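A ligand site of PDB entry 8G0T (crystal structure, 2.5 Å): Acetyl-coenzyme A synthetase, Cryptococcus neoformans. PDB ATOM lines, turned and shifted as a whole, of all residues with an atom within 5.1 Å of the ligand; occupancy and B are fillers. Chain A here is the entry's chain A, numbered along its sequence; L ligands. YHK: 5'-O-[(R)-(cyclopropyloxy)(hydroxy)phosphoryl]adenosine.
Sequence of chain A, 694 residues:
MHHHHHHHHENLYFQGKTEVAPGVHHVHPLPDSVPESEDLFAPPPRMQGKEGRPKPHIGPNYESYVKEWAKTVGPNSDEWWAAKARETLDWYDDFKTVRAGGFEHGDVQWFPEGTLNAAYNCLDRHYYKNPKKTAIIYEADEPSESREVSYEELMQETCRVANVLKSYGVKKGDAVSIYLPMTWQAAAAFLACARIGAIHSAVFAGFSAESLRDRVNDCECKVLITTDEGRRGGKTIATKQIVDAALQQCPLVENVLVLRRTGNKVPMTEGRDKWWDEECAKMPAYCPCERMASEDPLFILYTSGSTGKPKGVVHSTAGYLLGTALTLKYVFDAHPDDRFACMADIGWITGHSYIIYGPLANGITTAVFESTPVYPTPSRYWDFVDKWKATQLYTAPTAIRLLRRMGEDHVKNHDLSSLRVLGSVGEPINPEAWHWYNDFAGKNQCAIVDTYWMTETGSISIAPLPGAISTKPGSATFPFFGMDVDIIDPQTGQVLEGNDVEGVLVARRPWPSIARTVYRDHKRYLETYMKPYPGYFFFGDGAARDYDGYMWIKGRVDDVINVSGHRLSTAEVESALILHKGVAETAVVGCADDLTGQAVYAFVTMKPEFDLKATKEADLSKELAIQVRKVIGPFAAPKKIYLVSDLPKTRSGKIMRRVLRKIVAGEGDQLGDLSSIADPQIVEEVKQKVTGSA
OD2 of Asp 541 sits at hydrogen-bond distance from O1 of the ligand (3.0 Å).
An oxygen (O1) of the ligand sits at hydrogen-bond distance from the guanidinium group of Arg 556, 3.4 Å away.
The side-chain carboxylate (OD1) of Asp 450 lies within hydrogen-bond range of a nitrogen (N5) of the ligand (2.9 Å).
The side-chain amino group (NZ) of Lys 654 lies within salt-bridge range of an oxygen (O7) of the ligand.
N of Thr 455 lies within hydrogen-bond range of O6 of the ligand, 3.1 Å away.
The backbone NH (N) of Gly 426 sits at hydrogen-bond distance from a nitrogen (N2) of the ligand.
The side-chain sulfur (SD) of Met 454 lies close to an oxygen (O1) of the ligand, at 3.5 Å.
An oxygen (O7) of the ligand lies within hydrogen-bond range of the indole nitrogen (NE1) of Trp 348 (2.9 Å).
The backbone carbonyl oxygen (O) of Thr 451 sits at hydrogen-bond distance from a nitrogen (N5) of the ligand, 2.8 Å away.
An oxygen (O5) of the ligand lies within hydrogen-bond range of the side-chain hydroxyl (OG1) of Thr 455 (3.0 Å).
N of Thr 451 lies within hydrogen-bond range of O of Ser 424, at 2.8 Å.
NH1 of Arg 556 lies within hydrogen-bond range of O of Phe 539, at 3.2 Å.
The guanidinium group of Arg 556 is in salt-bridge range of the side-chain carboxylate of Asp 541 (3.7 Å).
A nitrogen (N3) of the ligand lies close to the backbone nitrogen (N) of Pro 428 (3.3 Å).
The backbone NH (N) of Tyr 452 lies close to a nitrogen (N5) of the ligand (3.3 Å).
Merely in contact with the ligand: Trp 453, Ile 349, Glu 427, Thr 350, Val 425 and Ile 553.
Hydrophobic or aromatic side chains that line the ligand: Trp 348, Ile 349, Val 425, Pro 428, Tyr 452, Trp 453, Met 454 and Ile 553.
Along chain A the residues within 4 Å of the ligand span positions 348 to 654.
The nearest printed residue that does not touch the ligand is Glu 456 (4.2 Å).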
ATOM      1  N   THR A 303     -24.321  -0.232  24.219  1.00  0.00           N
ATOM      2  CA  THR A 303     -24.796  -0.041  22.852  1.00  0.00           C
ATOM      3  C   THR A 303     -26.098  -0.789  22.634  1.00  0.00           C
ATOM      4  O   THR A 303     -26.259  -1.925  23.091  1.00  0.00           O
ATOM      5  CB  THR A 303     -23.752  -0.524  21.850  1.00  0.00           C
ATOM      6  OG1 THR A 303     -23.437  -1.896  22.107  1.00  0.00           O
ATOM      7  CG2 THR A 303     -22.488   0.323  21.939  1.00  0.00           C
ATOM      8  N   TRP A 348     -25.942   8.606  23.317  1.00  0.00           N
ATOM      9  CA  TRP A 348     -25.142   8.119  22.207  1.00  0.00           C
ATOM     10  C   TRP A 348     -23.693   8.547  22.424  1.00  0.00           C
ATOM     11  O   TRP A 348     -23.431   9.584  23.047  1.00  0.00           O
ATOM     12  CB  TRP A 348     -25.677   8.692  20.884  1.00  0.00           C
ATOM     13  CG  TRP A 348     -25.253   7.985  19.648  1.00  0.00           C
ATOM     14  CD1 TRP A 348     -24.699   6.740  19.539  1.00  0.00           C
ATOM     15  CD2 TRP A 348     -25.373   8.472  18.308  1.00  0.00           C
ATOM     16  NE1 TRP A 348     -24.459   6.438  18.227  1.00  0.00           N
ATOM     17  CE2 TRP A 348     -24.859   7.482  17.448  1.00  0.00           C
ATOM     18  CE3 TRP A 348     -25.864   9.662  17.747  1.00  0.00           C
ATOM     19  CZ2 TRP A 348     -24.829   7.638  16.066  1.00  0.00           C
ATOM     20  CZ3 TRP A 348     -25.829   9.817  16.379  1.00  0.00           C
ATOM     21  CH2 TRP A 348     -25.312   8.809  15.546  1.00  0.00           C
ATOM     22  N   ILE A 349     -22.763   7.747  21.916  1.00  0.00           N
ATOM     23  CA  ILE A 349     -21.360   8.137  22.048  1.00  0.00           C
ATOM     24  C   ILE A 349     -21.134   9.466  21.346  1.00  0.00           C
ATOM     25  O   ILE A 349     -20.278  10.251  21.769  1.00  0.00           O
ATOM     26  CB  ILE A 349     -20.445   7.033  21.485  1.00  0.00           C
ATOM     27  CG1 ILE A 349     -18.972   7.389  21.709  1.00  0.00           C
ATOM     28  CG2 ILE A 349     -20.707   6.806  20.008  1.00  0.00           C
ATOM     29  CD1 ILE A 349     -18.543   7.361  23.166  1.00  0.00           C
ATOM     30  N   THR A 350     -21.907   9.749  20.292  1.00  0.00           N
ATOM     31  CA  THR A 350     -21.812  11.052  19.622  1.00  0.00           C
ATOM     32  C   THR A 350     -22.093  12.181  20.596  1.00  0.00           C
ATOM     33  O   THR A 350     -21.443  13.238  20.534  1.00  0.00           O
ATOM     34  CB  THR A 350     -22.789  11.108  18.445  1.00  0.00           C
ATOM     35  OG1 THR A 350     -22.642   9.932  17.646  1.00  0.00           O
ATOM     36  CG2 THR A 350     -22.539  12.349  17.600  1.00  0.00           C
ATOM     37  N   SER A 424     -22.104  14.489   9.268  1.00  0.00           N
ATOM     38  CA  SER A 424     -23.013  13.362   9.254  1.00  0.00           C
ATOM     39  C   SER A 424     -22.363  12.190   9.992  1.00  0.00           C
ATOM     40  O   SER A 424     -21.165  11.941   9.812  1.00  0.00           O
ATOM     41  CB  SER A 424     -23.371  12.947   7.822  1.00  0.00           C
ATOM     42  OG  SER A 424     -24.349  11.922   7.810  1.00  0.00           O
ATOM     43  N   VAL A 425     -23.143  11.495  10.809  1.00  0.00           N
ATOM     44  CA  VAL A 425     -22.605  10.411  11.633  1.00  0.00           C
ATOM     45  C   VAL A 425     -23.702   9.406  11.931  1.00  0.00           C
ATOM     46  O   VAL A 425     -24.852   9.779  12.194  1.00  0.00           O
ATOM     47  CB  VAL A 425     -21.996  10.961  12.945  1.00  0.00           C
ATOM     48  CG1 VAL A 425     -23.049  11.708  13.759  1.00  0.00           C
ATOM     49  CG2 VAL A 425     -21.397   9.840  13.774  1.00  0.00           C
ATOM     50  N   GLY A 426     -23.335   8.119  11.919  1.00  0.00           N
ATOM     51  CA  GLY A 426     -24.235   7.041  12.290  1.00  0.00           C
ATOM     52  C   GLY A 426     -24.403   5.990  11.209  1.00  0.00           C
ATOM     53  O   GLY A 426     -24.621   4.815  11.518  1.00  0.00           O
ATOM     54  N   GLU A 427     -24.329   6.399   9.951  1.00  0.00           N
ATOM     55  CA  GLU A 427     -24.518   5.477   8.833  1.00  0.00           C
ATOM     56  C   GLU A 427     -23.986   6.141   7.584  1.00  0.00           C
ATOM     57  O   GLU A 427     -23.704   7.348   7.578  1.00  0.00           O
ATOM     58  CB  GLU A 427     -25.992   5.111   8.639  1.00  0.00           C
ATOM     59  CG  GLU A 427     -26.443   3.819   9.297  1.00  0.00           C
ATOM     60  CD  GLU A 427     -27.853   3.443   8.897  1.00  0.00           C
ATOM     61  OE1 GLU A 427     -28.511   4.260   8.211  1.00  0.00           O
ATOM     62  OE2 GLU A 427     -28.320   2.384   9.337  1.00  0.00           O
ATOM     63  N   PRO A 428     -23.804   5.379   6.501  1.00  0.00           N
ATOM     64  CA  PRO A 428     -23.501   6.013   5.221  1.00  0.00           C
ATOM     65  C   PRO A 428     -24.575   7.042   4.900  1.00  0.00           C
ATOM     66  O   PRO A 428     -25.752   6.848   5.205  1.00  0.00           O
ATOM     67  CB  PRO A 428     -23.517   4.845   4.232  1.00  0.00           C
ATOM     68  CG  PRO A 428     -23.288   3.624   5.069  1.00  0.00           C
ATOM     69  CD  PRO A 428     -23.904   3.916   6.398  1.00  0.00           C
ATOM     70  N   ASP A 450     -18.518  13.619   6.342  1.00  0.00           N
ATOM     71  CA  ASP A 450     -19.118  12.322   6.632  1.00  0.00           C
ATOM     72  C   ASP A 450     -18.190  11.596   7.588  1.00  0.00           C
ATOM     73  O   ASP A 450     -17.191  10.999   7.175  1.00  0.00           O
ATOM     74  CB  ASP A 450     -19.347  11.535   5.343  1.00  0.00           C
ATOM     75  CG  ASP A 450     -20.151  10.270   5.559  1.00  0.00           C
ATOM     76  OD1 ASP A 450     -20.760  10.124   6.641  1.00  0.00           O
ATOM     77  OD2 ASP A 450     -20.199   9.425   4.630  1.00  0.00           O
ATOM     78  N   THR A 451     -18.509  11.643   8.880  1.00  0.00           N
ATOM     79  CA  THR A 451     -17.622  11.145   9.913  1.00  0.00           C
ATOM     80  C   THR A 451     -17.944   9.682  10.225  1.00  0.00           C
ATOM     81  O   THR A 451     -19.035   9.380  10.709  1.00  0.00           O
ATOM     82  CB  THR A 451     -17.755  11.988  11.188  1.00  0.00           C
ATOM     83  OG1 THR A 451     -19.043  11.778  11.776  1.00  0.00           O
ATOM     84  CG2 THR A 451     -17.595  13.465  10.870  1.00  0.00           C
ATOM     85  N   TYR A 452     -16.994   8.803   9.945  1.00  0.00           N
ATOM     86  CA  TYR A 452     -17.136   7.387  10.254  1.00  0.00           C
ATOM     87  C   TYR A 452     -16.351   7.052  11.511  1.00  0.00           C
ATOM     88  O   TYR A 452     -15.182   7.443  11.661  1.00  0.00           O
ATOM     89  CB  TYR A 452     -16.641   6.507   9.099  1.00  0.00           C
ATOM     90  CG  TYR A 452     -16.512   5.065   9.510  1.00  0.00           C
ATOM     91  CD1 TYR A 452     -17.642   4.255   9.647  1.00  0.00           C
ATOM     92  CD2 TYR A 452     -15.273   4.503   9.790  1.00  0.00           C
ATOM     93  CE1 TYR A 452     -17.523   2.933  10.033  1.00  0.00           C
ATOM     94  CE2 TYR A 452     -15.151   3.193  10.184  1.00  0.00           C
ATOM     95  CZ  TYR A 452     -16.273   2.416  10.305  1.00  0.00           C
ATOM     96  OH  TYR A 452     -16.143   1.102  10.687  1.00  0.00           O
ATOM     97  N   TRP A 453     -16.983   6.323  12.414  1.00  0.00           N
ATOM     98  CA  TRP A 453     -16.344   5.806  13.629  1.00  0.00           C
ATOM     99  C   TRP A 453     -17.342   4.917  14.345  1.00  0.00           C
ATOM    100  O   TRP A 453     -18.421   4.618  13.813  1.00  0.00           O
ATOM    101  CB  TRP A 453     -15.837   6.945  14.517  1.00  0.00           C
ATOM    102  CG  TRP A 453     -16.864   7.975  14.904  1.00  0.00           C
ATOM    103  CD1 TRP A 453     -17.577   8.772  14.055  1.00  0.00           C
ATOM    104  CD2 TRP A 453     -17.250   8.343  16.229  1.00  0.00           C
ATOM    105  NE1 TRP A 453     -18.397   9.600  14.774  1.00  0.00           N
ATOM    106  CE2 TRP A 453     -18.227   9.360  16.106  1.00  0.00           C
ATOM    107  CE3 TRP A 453     -16.893   7.907  17.508  1.00  0.00           C
ATOM    108  CZ2 TRP A 453     -18.832   9.937  17.218  1.00  0.00           C
ATOM    109  CZ3 TRP A 453     -17.486   8.484  18.600  1.00  0.00           C
ATOM    110  CH2 TRP A 453     -18.454   9.489  18.450  1.00  0.00           C
ATOM    111  N   MET A 454     -16.971   4.475  15.543  1.00  0.00           N
ATOM    112  CA  MET A 454     -17.771   3.582  16.344  1.00  0.00           C
ATOM    113  C   MET A 454     -17.686   3.983  17.808  1.00  0.00           C
ATOM    114  O   MET A 454     -16.794   4.735  18.216  1.00  0.00           O
ATOM    115  CB  MET A 454     -17.295   2.127  16.181  1.00  0.00           C
ATOM    116  CG  MET A 454     -17.518   1.557  14.816  1.00  0.00           C
ATOM    117  SD  MET A 454     -16.827  -0.095  14.574  1.00  0.00           S
ATOM    118  CE  MET A 454     -15.952  -0.416  16.086  1.00  0.00           C
ATOM    119  N   THR A 455     -18.630   3.464  18.593  1.00  0.00           N
ATOM    120  CA  THR A 455     -18.536   3.600  20.042  1.00  0.00           C
ATOM    121  C   THR A 455     -17.231   3.022  20.553  1.00  0.00           C
ATOM    122  O   THR A 455     -16.649   3.550  21.511  1.00  0.00           O
ATOM    123  CB  THR A 455     -19.727   2.901  20.700  1.00  0.00           C
ATOM    124  OG1 THR A 455     -20.951   3.446  20.179  1.00  0.00           O
ATOM    125  CG2 THR A 455     -19.687   3.069  22.216  1.00  0.00           C
ATOM    126  N   GLU A 456     -16.736   1.968  19.914  1.00  0.00           N
ATOM    127  CA  GLU A 456     -15.495   1.319  20.292  1.00  0.00           C
ATOM    128  C   GLU A 456     -14.251   2.073  19.838  1.00  0.00           C
ATOM    129  O   GLU A 456     -13.153   1.748  20.293  1.00  0.00           O
ATOM    130  CB  GLU A 456     -15.460  -0.112  19.734  1.00  0.00           C
ATOM    131  CG  GLU A 456     -16.555  -1.012  20.289  1.00  0.00           C
ATOM    132  CD  GLU A 456     -17.860  -0.895  19.517  1.00  0.00           C
ATOM    133  OE1 GLU A 456     -18.077   0.147  18.866  1.00  0.00           O
ATOM    134  OE2 GLU A 456     -18.675  -1.843  19.572  1.00  0.00           O
ATOM    135  N   ALA A 476     -16.423   8.700   3.397  1.00  0.00           N
ATOM    136  CA  ALA A 476     -15.704   9.134   4.585  1.00  0.00           C
ATOM    137  C   ALA A 476     -14.304   9.635   4.250  1.00  0.00           C
ATOM    138  O   ALA A 476     -13.664  10.264   5.104  1.00  0.00           O
ATOM    139  CB  ALA A 476     -15.616   7.987   5.584  1.00  0.00           C
ATOM    140  N   PHE A 539     -13.501  -3.587  12.740  1.00  0.00           N
ATOM    141  CA  PHE A 539     -14.650  -2.705  12.897  1.00  0.00           C
ATOM    142  C   PHE A 539     -15.980  -3.423  12.683  1.00  0.00           C
ATOM    143  O   PHE A 539     -16.980  -3.066  13.305  1.00  0.00           O
ATOM    144  CB  PHE A 539     -14.561  -1.529  11.910  1.00  0.00           C
ATOM    145  CG  PHE A 539     -13.422  -0.588  12.165  1.00  0.00           C
ATOM    146  CD1 PHE A 539     -12.173  -0.828  11.604  1.00  0.00           C
ATOM    147  CD2 PHE A 539     -13.607   0.551  12.930  1.00  0.00           C
ATOM    148  CE1 PHE A 539     -11.123   0.053  11.842  1.00  0.00           C
ATOM    149  CE2 PHE A 539     -12.569   1.417  13.156  1.00  0.00           C
ATOM    150  CZ  PHE A 539     -11.315   1.176  12.609  1.00  0.00           C
ATOM    151  N   ASP A 541     -17.228  -3.543   9.470  1.00  0.00           N
ATOM    152  CA  ASP A 541     -17.791  -2.807   8.350  1.00  0.00           C
ATOM    153  C   ASP A 541     -17.120  -3.219   7.053  1.00  0.00           C
ATOM    154  O   ASP A 541     -15.894  -3.394   7.004  1.00  0.00           O
ATOM    155  CB  ASP A 541     -17.617  -1.305   8.550  1.00  0.00           C
ATOM    156  CG  ASP A 541     -18.593  -0.739   9.526  1.00  0.00           C
ATOM    157  OD1 ASP A 541     -19.780  -1.109   9.474  1.00  0.00           O
ATOM    158  OD2 ASP A 541     -18.174   0.089  10.362  1.00  0.00           O
ATOM    159  N   ILE A 553     -17.103   3.629   3.185  1.00  0.00           N
ATOM    160  CA  ILE A 553     -17.661   2.715   4.176  1.00  0.00           C
ATOM    161  C   ILE A 553     -19.095   2.448   3.762  1.00  0.00           C
ATOM    162  O   ILE A 553     -19.971   3.308   3.930  1.00  0.00           O
ATOM    163  CB  ILE A 553     -17.586   3.304   5.589  1.00  0.00           C
ATOM    164  CG1 ILE A 553     -16.164   3.786   5.895  1.00  0.00           C
ATOM    165  CG2 ILE A 553     -18.031   2.279   6.614  1.00  0.00           C
ATOM    166  CD1 ILE A 553     -15.088   2.716   5.744  1.00  0.00           C
ATOM    167  N   ARG A 556     -22.505  -2.424   7.184  1.00  0.00           N
ATOM    168  CA  ARG A 556     -22.054  -3.520   8.039  1.00  0.00           C
ATOM    169  C   ARG A 556     -21.742  -4.758   7.212  1.00  0.00           C
ATOM    170  O   ARG A 556     -22.369  -5.018   6.184  1.00  0.00           O
ATOM    171  CB  ARG A 556     -23.114  -3.850   9.091  1.00  0.00           C
ATOM    172  CG  ARG A 556     -23.422  -2.727  10.075  1.00  0.00           C
ATOM    173  CD  ARG A 556     -22.264  -2.442  11.021  1.00  0.00           C
ATOM    174  NE  ARG A 556     -21.920  -3.577  11.875  1.00  0.00           N
ATOM    175  CZ  ARG A 556     -20.903  -3.586  12.724  1.00  0.00           C
ATOM    176  NH1 ARG A 556     -20.099  -2.540  12.846  1.00  0.00           N
ATOM    177  NH2 ARG A 556     -20.682  -4.674  13.460  1.00  0.00           N
ATOM    178  N   SER A 652     -30.376   6.230  18.185  1.00  0.00           N
ATOM    179  CA  SER A 652     -29.340   7.035  17.546  1.00  0.00           C
ATOM    180  C   SER A 652     -29.641   7.311  16.076  1.00  0.00           C
ATOM    181  O   SER A 652     -29.091   8.272  15.523  1.00  0.00           O
ATOM    182  CB  SER A 652     -27.992   6.344  17.670  1.00  0.00           C
ATOM    183  OG  SER A 652     -28.033   5.036  17.112  1.00  0.00           O
ATOM    184  N   LYS A 654     -29.692   4.597  13.588  1.00  0.00           N
ATOM    185  CA  LYS A 654     -29.257   3.531  12.706  1.00  0.00           C
ATOM    186  C   LYS A 654     -30.437   2.641  12.319  1.00  0.00           C
ATOM    187  O   LYS A 654     -31.312   2.357  13.133  1.00  0.00           O
ATOM    188  CB  LYS A 654     -28.158   2.684  13.356  1.00  0.00           C
ATOM    189  CG  LYS A 654     -26.815   3.383  13.458  1.00  0.00           C
ATOM    190  CD  LYS A 654     -25.710   2.432  13.901  1.00  0.00           C
ATOM    191  CE  LYS A 654     -25.801   2.082  15.374  1.00  0.00           C
ATOM    192  NZ  LYS A 654     -24.622   1.289  15.833  1.00  0.00           N
HETATM  193  C1  YHK L   1     -20.323   2.041  12.304  1.00  0.00           C
HETATM  194  C10 YHK L   1     -21.142   3.171  14.450  1.00  0.00           C
HETATM  195  C11 YHK L   1     -21.545   5.876  16.380  1.00  0.00           C
HETATM  196  C12 YHK L   1     -20.768   6.553  15.291  1.00  0.00           C
HETATM  197  C13 YHK L   1     -20.776   7.128  16.666  1.00  0.00           C
HETATM  198  C2  YHK L   1     -21.044   1.901  10.958  1.00  0.00           C
HETATM  199  C3  YHK L   1     -21.994   3.095  11.019  1.00  0.00           C
HETATM  200  C4  YHK L   1     -21.120   5.429  11.499  1.00  0.00           C
HETATM  201  C5  YHK L   1     -20.634   6.115   9.543  1.00  0.00           C
HETATM  202  C6  YHK L   1     -21.126   4.830   9.394  1.00  0.00           C
HETATM  203  C7  YHK L   1     -20.856   4.907   7.208  1.00  0.00           C
HETATM  204  C8  YHK L   1     -20.249   6.799   8.380  1.00  0.00           C
HETATM  205  C9  YHK L   1     -21.505   2.398  13.212  1.00  0.00           C
HETATM  206  N1  YHK L   1     -21.427   4.394  10.658  1.00  0.00           N
HETATM  207  N2  YHK L   1     -20.646   6.484  10.882  1.00  0.00           N
HETATM  208  N3  YHK L   1     -21.262   4.166   8.239  1.00  0.00           N
HETATM  209  N4  YHK L   1     -20.375   6.148   7.199  1.00  0.00           N
HETATM  210  N5  YHK L   1     -19.760   8.043   8.376  1.00  0.00           N
HETATM  211  O1  YHK L   1     -19.725   0.845  12.772  1.00  0.00           O
HETATM  212  O2  YHK L   1     -22.416   3.169  12.381  1.00  0.00           O
HETATM  213  O3  YHK L   1     -21.759   0.684  10.865  1.00  0.00           O
HETATM  214  O4  YHK L   1     -22.283   3.241  15.321  1.00  0.00           O
HETATM  215  O5  YHK L   1     -21.379   2.292  17.448  1.00  0.00           O
HETATM  216  O6  YHK L   1     -20.971   4.707  16.912  1.00  0.00           O
HETATM  217  O7  YHK L   1     -23.300   3.935  17.500  1.00  0.00           O
HETATM  218  P1  YHK L   1     -22.024   3.499  16.884  1.00  0.00           P
